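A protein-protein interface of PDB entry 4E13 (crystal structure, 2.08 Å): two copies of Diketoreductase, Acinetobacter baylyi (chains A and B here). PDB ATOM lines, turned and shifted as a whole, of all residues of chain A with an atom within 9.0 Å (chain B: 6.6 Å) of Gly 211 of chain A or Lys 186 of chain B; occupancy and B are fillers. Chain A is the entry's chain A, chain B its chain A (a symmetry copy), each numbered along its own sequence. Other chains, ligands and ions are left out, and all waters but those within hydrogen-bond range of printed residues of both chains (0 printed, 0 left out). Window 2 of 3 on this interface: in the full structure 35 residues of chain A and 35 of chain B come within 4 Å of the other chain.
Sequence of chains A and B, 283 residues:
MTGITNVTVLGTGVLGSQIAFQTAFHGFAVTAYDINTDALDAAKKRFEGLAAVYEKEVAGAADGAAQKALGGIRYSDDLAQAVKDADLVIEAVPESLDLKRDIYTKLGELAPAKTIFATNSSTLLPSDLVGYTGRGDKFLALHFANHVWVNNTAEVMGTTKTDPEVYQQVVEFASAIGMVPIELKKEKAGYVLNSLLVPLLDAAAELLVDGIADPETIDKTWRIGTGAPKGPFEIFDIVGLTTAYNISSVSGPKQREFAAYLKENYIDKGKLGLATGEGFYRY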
ATOM      1  N   ALA A 204      12.937 -19.635  11.428  1.00  0.00           N
ATOM      2  CA  ALA A 204      11.612 -19.321  10.906  1.00  0.00           C
ATOM      3  C   ALA A 204      11.244 -17.875  11.254  1.00  0.00           C
ATOM      4  O   ALA A 204      10.727 -17.133  10.409  1.00  0.00           O
ATOM      5  CB  ALA A 204      10.568 -20.283  11.479  1.00  0.00           C
ATOM      6  N   ALA A 205      11.502 -17.482  12.502  1.00  0.00           N
ATOM      7  CA  ALA A 205      11.162 -16.125  12.945  1.00  0.00           C
ATOM      8  C   ALA A 205      11.857 -15.078  12.064  1.00  0.00           C
ATOM      9  O   ALA A 205      11.223 -14.123  11.605  1.00  0.00           O
ATOM     10  CB  ALA A 205      11.520 -15.928  14.404  1.00  0.00           C
ATOM     11  N   GLU A 206      13.149 -15.286  11.807  1.00  0.00           N
ATOM     12  CA  GLU A 206      13.927 -14.387  10.956  1.00  0.00           C
ATOM     13  C   GLU A 206      13.301 -14.245   9.584  1.00  0.00           C
ATOM     14  O   GLU A 206      13.151 -13.128   9.082  1.00  0.00           O
ATOM     15  CB  GLU A 206      15.379 -14.869  10.836  1.00  0.00           C
ATOM     16  CG  GLU A 206      16.279 -14.023   9.918  1.00  0.00           C
ATOM     17  CD  GLU A 206      15.990 -14.219   8.434  1.00  0.00           C
ATOM     18  OE1 GLU A 206      16.359 -13.338   7.625  1.00  0.00           O
ATOM     19  OE2 GLU A 206      15.400 -15.260   8.071  1.00  0.00           O
ATOM     20  N   LEU A 207      12.936 -15.367   8.967  1.00  0.00           N
ATOM     21  CA  LEU A 207      12.290 -15.319   7.662  1.00  0.00           C
ATOM     22  C   LEU A 207      11.026 -14.475   7.698  1.00  0.00           C
ATOM     23  O   LEU A 207      10.726 -13.762   6.735  1.00  0.00           O
ATOM     24  CB  LEU A 207      11.933 -16.725   7.160  1.00  0.00           C
ATOM     25  CG  LEU A 207      13.091 -17.676   6.865  1.00  0.00           C
ATOM     26  CD1 LEU A 207      12.545 -19.034   6.416  1.00  0.00           C
ATOM     27  CD2 LEU A 207      13.960 -17.068   5.769  1.00  0.00           C
ATOM     28  N   LEU A 208      10.269 -14.572   8.791  1.00  0.00           N
ATOM     29  CA  LEU A 208       9.010 -13.848   8.877  1.00  0.00           C
ATOM     30  C   LEU A 208       9.264 -12.357   9.083  1.00  0.00           C
ATOM     31  O   LEU A 208       8.739 -11.527   8.339  1.00  0.00           O
ATOM     32  CB  LEU A 208       8.124 -14.393  10.007  1.00  0.00           C
ATOM     33  CG  LEU A 208       6.749 -13.728  10.171  1.00  0.00           C
ATOM     34  CD1 LEU A 208       5.923 -13.858   8.901  1.00  0.00           C
ATOM     35  CD2 LEU A 208       6.012 -14.341  11.348  1.00  0.00           C
ATOM     36  N   VAL A 209      10.079 -12.031  10.083  1.00  0.00           N
ATOM     37  CA  VAL A 209      10.361 -10.642  10.423  1.00  0.00           C
ATOM     38  C   VAL A 209      10.954  -9.889   9.239  1.00  0.00           C
ATOM     39  O   VAL A 209      10.496  -8.797   8.900  1.00  0.00           O
ATOM     40  CB  VAL A 209      11.334 -10.536  11.601  1.00  0.00           C
ATOM     41  CG1 VAL A 209      11.667  -9.084  11.864  1.00  0.00           C
ATOM     42  CG2 VAL A 209      10.725 -11.150  12.845  1.00  0.00           C
ATOM     43  N   ASP A 210      11.962 -10.477   8.602  1.00  0.00           N
ATOM     44  CA  ASP A 210      12.651  -9.819   7.497  1.00  0.00           C
ATOM     45  C   ASP A 210      11.806  -9.776   6.244  1.00  0.00           C
ATOM     46  O   ASP A 210      12.269  -9.334   5.190  1.00  0.00           O
ATOM     47  CB  ASP A 210      13.997 -10.487   7.229  1.00  0.00           C
ATOM     48  CG  ASP A 210      14.951 -10.335   8.398  1.00  0.00           C
ATOM     49  OD1 ASP A 210      14.716  -9.428   9.232  1.00  0.00           O
ATOM     50  OD2 ASP A 210      15.928 -11.110   8.495  1.00  0.00           O
ATOM     51  N   GLY A 211      10.564 -10.230   6.353  1.00  0.00           N
ATOM     52  CA  GLY A 211       9.649 -10.154   5.229  1.00  0.00           C
ATOM     53  C   GLY A 211       9.962 -11.083   4.064  1.00  0.00           C
ATOM     54  O   GLY A 211       9.551 -10.804   2.934  1.00  0.00           O
ATOM     55  N   ILE A 212      10.663 -12.186   4.323  1.00  0.00           N
ATOM     56  CA  ILE A 212      11.000 -13.129   3.250  1.00  0.00           C
ATOM     57  C   ILE A 212       9.804 -13.982   2.825  1.00  0.00           C
ATOM     58  O   ILE A 212       9.659 -14.308   1.644  1.00  0.00           O
ATOM     59  CB  ILE A 212      12.130 -14.091   3.646  1.00  0.00           C
ATOM     60  CG1 ILE A 212      13.366 -13.309   4.085  1.00  0.00           C
ATOM     61  CG2 ILE A 212      12.479 -14.989   2.460  1.00  0.00           C
ATOM     62  CD1 ILE A 212      13.905 -12.382   3.013  1.00  0.00           C
ATOM     63  N   ALA A 213       8.962 -14.371   3.780  1.00  0.00           N
ATOM     64  CA  ALA A 213       7.809 -15.214   3.461  1.00  0.00           C
ATOM     65  C   ALA A 213       6.821 -15.256   4.618  1.00  0.00           C
ATOM     66  O   ALA A 213       7.201 -15.065   5.775  1.00  0.00           O
ATOM     67  CB  ALA A 213       8.279 -16.625   3.134  1.00  0.00           C
ATOM     68  N   ASP A 214       5.560 -15.536   4.310  1.00  0.00           N
ATOM     69  CA  ASP A 214       4.526 -15.603   5.337  1.00  0.00           C
ATOM     70  C   ASP A 214       4.535 -16.956   6.074  1.00  0.00           C
ATOM     71  O   ASP A 214       5.097 -17.942   5.587  1.00  0.00           O
ATOM     72  CB  ASP A 214       3.155 -15.274   4.744  1.00  0.00           C
ATOM     73  CG  ASP A 214       2.716 -16.268   3.715  1.00  0.00           C
ATOM     74  OD1 ASP A 214       1.735 -15.978   3.002  1.00  0.00           O
ATOM     75  OD2 ASP A 214       3.338 -17.345   3.628  1.00  0.00           O
ATOM     76  N   ILE A 218       6.242 -20.730   5.030  1.00  0.00           N
ATOM     77  CA  ILE A 218       7.340 -21.281   5.800  1.00  0.00           C
ATOM     78  C   ILE A 218       6.944 -22.651   6.357  1.00  0.00           C
ATOM     79  O   ILE A 218       7.735 -23.599   6.325  1.00  0.00           O
ATOM     80  CB  ILE A 218       7.735 -20.319   6.956  1.00  0.00           C
ATOM     81  CG1 ILE A 218       8.155 -18.961   6.371  1.00  0.00           C
ATOM     82  CG2 ILE A 218       8.854 -20.913   7.779  1.00  0.00           C
ATOM     83  CD1 ILE A 218       8.511 -17.901   7.409  1.00  0.00           C
ATOM     84  N   LYS A 254      18.130 -10.059  16.461  1.00  0.00           N
ATOM     85  CA  LYS A 254      17.126 -10.509  15.505  1.00  0.00           C
ATOM     86  C   LYS A 254      15.906 -11.107  16.202  1.00  0.00           C
ATOM     87  O   LYS A 254      14.767 -10.818  15.824  1.00  0.00           O
ATOM     88  CB  LYS A 254      17.711 -11.478  14.481  1.00  0.00           C
ATOM     89  CG  LYS A 254      16.683 -11.970  13.481  1.00  0.00           C
ATOM     90  CD  LYS A 254      15.989 -10.815  12.751  1.00  0.00           C
ATOM     91  CE  LYS A 254      16.959 -10.013  11.900  1.00  0.00           C
ATOM     92  NZ  LYS A 254      16.256  -8.917  11.176  1.00  0.00           N
ATOM     93  N   GLU A 257      13.736  -8.598  17.652  1.00  0.00           N
ATOM     94  CA  GLU A 257      12.926  -8.014  16.606  1.00  0.00           C
ATOM     95  C   GLU A 257      11.651  -8.861  16.432  1.00  0.00           C
ATOM     96  O   GLU A 257      10.570  -8.339  16.138  1.00  0.00           O
ATOM     97  CB  GLU A 257      13.750  -7.940  15.325  1.00  0.00           C
ATOM     98  CG  GLU A 257      13.137  -7.146  14.193  1.00  0.00           C
ATOM     99  CD  GLU A 257      14.158  -6.861  13.093  1.00  0.00           C
ATOM    100  OE1 GLU A 257      15.373  -7.041  13.348  1.00  0.00           O
ATOM    101  OE2 GLU A 257      13.752  -6.453  11.981  1.00  0.00           O
ATOM    102  N   TYR A 261       7.609  -8.195  17.267  1.00  0.00           N
ATOM    103  CA  TYR A 261       6.660  -8.602  16.233  1.00  0.00           C
ATOM    104  C   TYR A 261       5.491  -9.399  16.836  1.00  0.00           C
ATOM    105  O   TYR A 261       4.330  -9.164  16.496  1.00  0.00           O
ATOM    106  CB  TYR A 261       7.377  -9.433  15.164  1.00  0.00           C
ATOM    107  CG  TYR A 261       6.493  -9.845  14.015  1.00  0.00           C
ATOM    108  CD1 TYR A 261       6.415  -9.064  12.867  1.00  0.00           C
ATOM    109  CD2 TYR A 261       5.735 -11.016  14.071  1.00  0.00           C
ATOM    110  CE1 TYR A 261       5.604  -9.432  11.797  1.00  0.00           C
ATOM    111  CE2 TYR A 261       4.916 -11.398  13.004  1.00  0.00           C
ATOM    112  CZ  TYR A 261       4.857 -10.600  11.872  1.00  0.00           C
ATOM    113  OH  TYR A 261       4.058 -10.956  10.810  1.00  0.00           O
ATOM    114  N   MET B 157      12.088 -16.913  -6.149  1.00  0.00           N
ATOM    115  CA  MET B 157      12.742 -15.812  -5.450  1.00  0.00           C
ATOM    116  C   MET B 157      13.356 -14.837  -6.452  1.00  0.00           C
ATOM    117  O   MET B 157      14.337 -15.170  -7.123  1.00  0.00           O
ATOM    118  CB  MET B 157      13.827 -16.371  -4.533  1.00  0.00           C
ATOM    119  CG  MET B 157      14.477 -15.347  -3.650  1.00  0.00           C
ATOM    120  SD  MET B 157      15.737 -16.082  -2.618  1.00  0.00           S
ATOM    121  CE  MET B 157      16.998 -16.433  -3.846  1.00  0.00           C
ATOM    122  N   GLY B 158      12.772 -13.642  -6.558  1.00  0.00           N
ATOM    123  CA  GLY B 158      13.279 -12.648  -7.492  1.00  0.00           C
ATOM    124  C   GLY B 158      14.191 -11.588  -6.886  1.00  0.00           C
ATOM    125  O   GLY B 158      14.556 -11.654  -5.710  1.00  0.00           O
ATOM    126  N   LEU B 184       8.907 -16.667  -2.237  1.00  0.00           N
ATOM    127  CA  LEU B 184       9.646 -15.708  -1.425  1.00  0.00           C
ATOM    128  C   LEU B 184       9.393 -14.271  -1.894  1.00  0.00           C
ATOM    129  O   LEU B 184       9.185 -14.022  -3.084  1.00  0.00           O
ATOM    130  CB  LEU B 184      11.144 -16.016  -1.381  1.00  0.00           C
ATOM    131  CG  LEU B 184      11.557 -17.293  -0.650  1.00  0.00           C
ATOM    132  CD1 LEU B 184      11.095 -18.523  -1.421  1.00  0.00           C
ATOM    133  CD2 LEU B 184      13.069 -17.318  -0.482  1.00  0.00           C
ATOM    134  N   LYS B 185       9.405 -13.337  -0.944  1.00  0.00           N
ATOM    135  CA  LYS B 185       9.040 -11.939  -1.192  1.00  0.00           C
ATOM    136  C   LYS B 185      10.280 -11.085  -1.429  1.00  0.00           C
ATOM    137  O   LYS B 185      10.282 -10.179  -2.264  1.00  0.00           O
ATOM    138  CB  LYS B 185       8.295 -11.399   0.025  1.00  0.00           C
ATOM    139  CG  LYS B 185       7.083 -12.229   0.399  1.00  0.00           C
ATOM    140  CD  LYS B 185       6.448 -11.735   1.684  1.00  0.00           C
ATOM    141  CE  LYS B 185       5.220 -12.558   2.023  1.00  0.00           C
ATOM    142  NZ  LYS B 185       4.219 -12.508   0.920  1.00  0.00           N
ATOM    143  N   LYS B 186      11.325 -11.377  -0.667  1.00  0.00           N
ATOM    144  CA  LYS B 186      12.606 -10.701  -0.799  1.00  0.00           C
ATOM    145  C   LYS B 186      13.670 -11.769  -0.970  1.00  0.00           C
ATOM    146  O   LYS B 186      13.494 -12.912  -0.539  1.00  0.00           O
ATOM    147  CB  LYS B 186      12.924  -9.898   0.468  1.00  0.00           C
ATOM    148  CG  LYS B 186      11.897  -8.840   0.835  1.00  0.00           C
ATOM    149  CD  LYS B 186      12.290  -8.124   2.127  1.00  0.00           C
ATOM    150  CE  LYS B 186      11.265  -7.059   2.513  1.00  0.00           C
ATOM    151  NZ  LYS B 186      11.628  -6.341   3.773  1.00  0.00           N
ATOM    152  N   GLU B 187      14.779 -11.398  -1.585  1.00  0.00           N
ATOM    153  CA  GLU B 187      15.866 -12.332  -1.786  1.00  0.00           C
ATOM    154  C   GLU B 187      16.376 -12.840  -0.428  1.00  0.00           C
ATOM    155  O   GLU B 187      16.309 -12.127   0.577  1.00  0.00           O
ATOM    156  CB  GLU B 187      16.966 -11.641  -2.602  1.00  0.00           C
ATOM    157  CG  GLU B 187      18.117 -12.529  -3.035  1.00  0.00           C
ATOM    158  CD  GLU B 187      18.905 -11.923  -4.187  1.00  0.00           C
ATOM    159  OE1 GLU B 187      18.379 -10.999  -4.855  1.00  0.00           O
ATOM    160  OE2 GLU B 187      20.043 -12.374  -4.431  1.00  0.00           O
ATOM    161  N   LYS B 188      16.863 -14.078  -0.398  1.00  0.00           N
ATOM    162  CA  LYS B 188      17.374 -14.687   0.827  1.00  0.00           C
ATOM    163  C   LYS B 188      18.311 -15.831   0.476  1.00  0.00           C
ATOM    164  O   LYS B 188      17.955 -16.714  -0.307  1.00  0.00           O
ATOM    165  CB  LYS B 188      16.205 -15.215   1.685  1.00  0.00           C
ATOM    166  CG  LYS B 188      16.609 -15.980   2.960  1.00  0.00           C
ATOM    167  CD  LYS B 188      17.329 -15.089   3.964  1.00  0.00           C
ATOM    168  CE  LYS B 188      17.805 -15.860   5.189  1.00  0.00           C
ATOM    169  NZ  LYS B 188      18.816 -16.894   4.858  1.00  0.00           N
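The backbone carbonyl oxygen of Leu 207 of chain A sits at hydrogen-bond distance from the backbone NH of Ile 212 of chain A (2.9 Å). O of Leu 207 of chain A sits at hydrogen-bond distance from N of Ala 213 of chain A, at 3.5 Å. OD1 of Asp 210 of chain A is in salt-bridge range of NZ of Lys 254 of chain A (2.5 Å). The side-chain carboxylate (OD2) of Asp 210 of chain A sits close to the side-chain carboxylate (OE1) of Glu 206 of chain A (2.4 Å). SD of Met 157 of chain B is in hydrogen-bond range of N of Lys 188 of chain B.
Among the printed residues, merely in contact across the chains: Glu 206 of chain A with Lys 188 of chain B (3.8 Å), Gly 211 of chain A with Lys 185 of chain B (3.2 Å), Gly 211 of chain A with Lys 186 of chain B (3.7 Å), Ile 212 of chain A with Leu 184 of chain B (3.4 Å), Ile 212 of chain A with Lys 186 of chain B (3.6 Å), Ile 212 of chain A with Glu 187 of chain B (3.4 Å), Ile 212 of chain A with Lys 188 of chain B (3.8 Å), Ala 213 of chain A with Lys 185 of chain B (3.98 Å) and Asp 214 of chain A with Lys 185 of chain B (3.8 Å).
The backbone carbonyl oxygen of Asp 210 of chain A sits close to the side-chain amino group of Lys 186 of chain B (3.4 Å). The backbone carbonyl oxygen of Ile 212 of chain A sits at hydrogen-bond distance from the backbone NH of Lys 185 of chain B.
No position is printed for both chains. Of the 11 pairs that touch across the chains among the printed residues, none has its exchanged pair printed and touching as well.
Hydrophobic or aromatic side chains of chain B that line the printed part of chain A: Leu 184. Among the printed residues, no Asp or Glu carboxylate lies within 4 Å of a Lys or Arg side-chain nitrogen of the other chain.
Of the printed residues of chain B, Glu 206 of chain A touches Lys 188 (3.8 Å). Printed residues of chain B within 4 Å of Asp 210 of chain A: Lys 186 (3.3 Å). Of chain B, only Lys 185 and Lys 186 come within 4 Å of Gly 211 of chain A. Printed residues of chain B within 4 Å of Ala 213 of chain A: Lys 185 (3.98 Å). Printed residues of chain B within 4 Å of Asp 214 of chain A: Lys 185 (3.8 Å). Tyr 261 of chain A touches none of the printed residues of chain B. Lys 186 of chain B touches three residues of chain A. Printed residues of chain A within 4 Å of Glu 187 of chain B: Ile 212 (3.4 Å). The nearest residue of chain B that does not touch Gly 211 of chain A is Leu 184 of chain B (5.9 Å). The nearest printed residue of chain A that does not touch Lys 188 of chain B is Leu 207 of chain A (4.01 Å).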
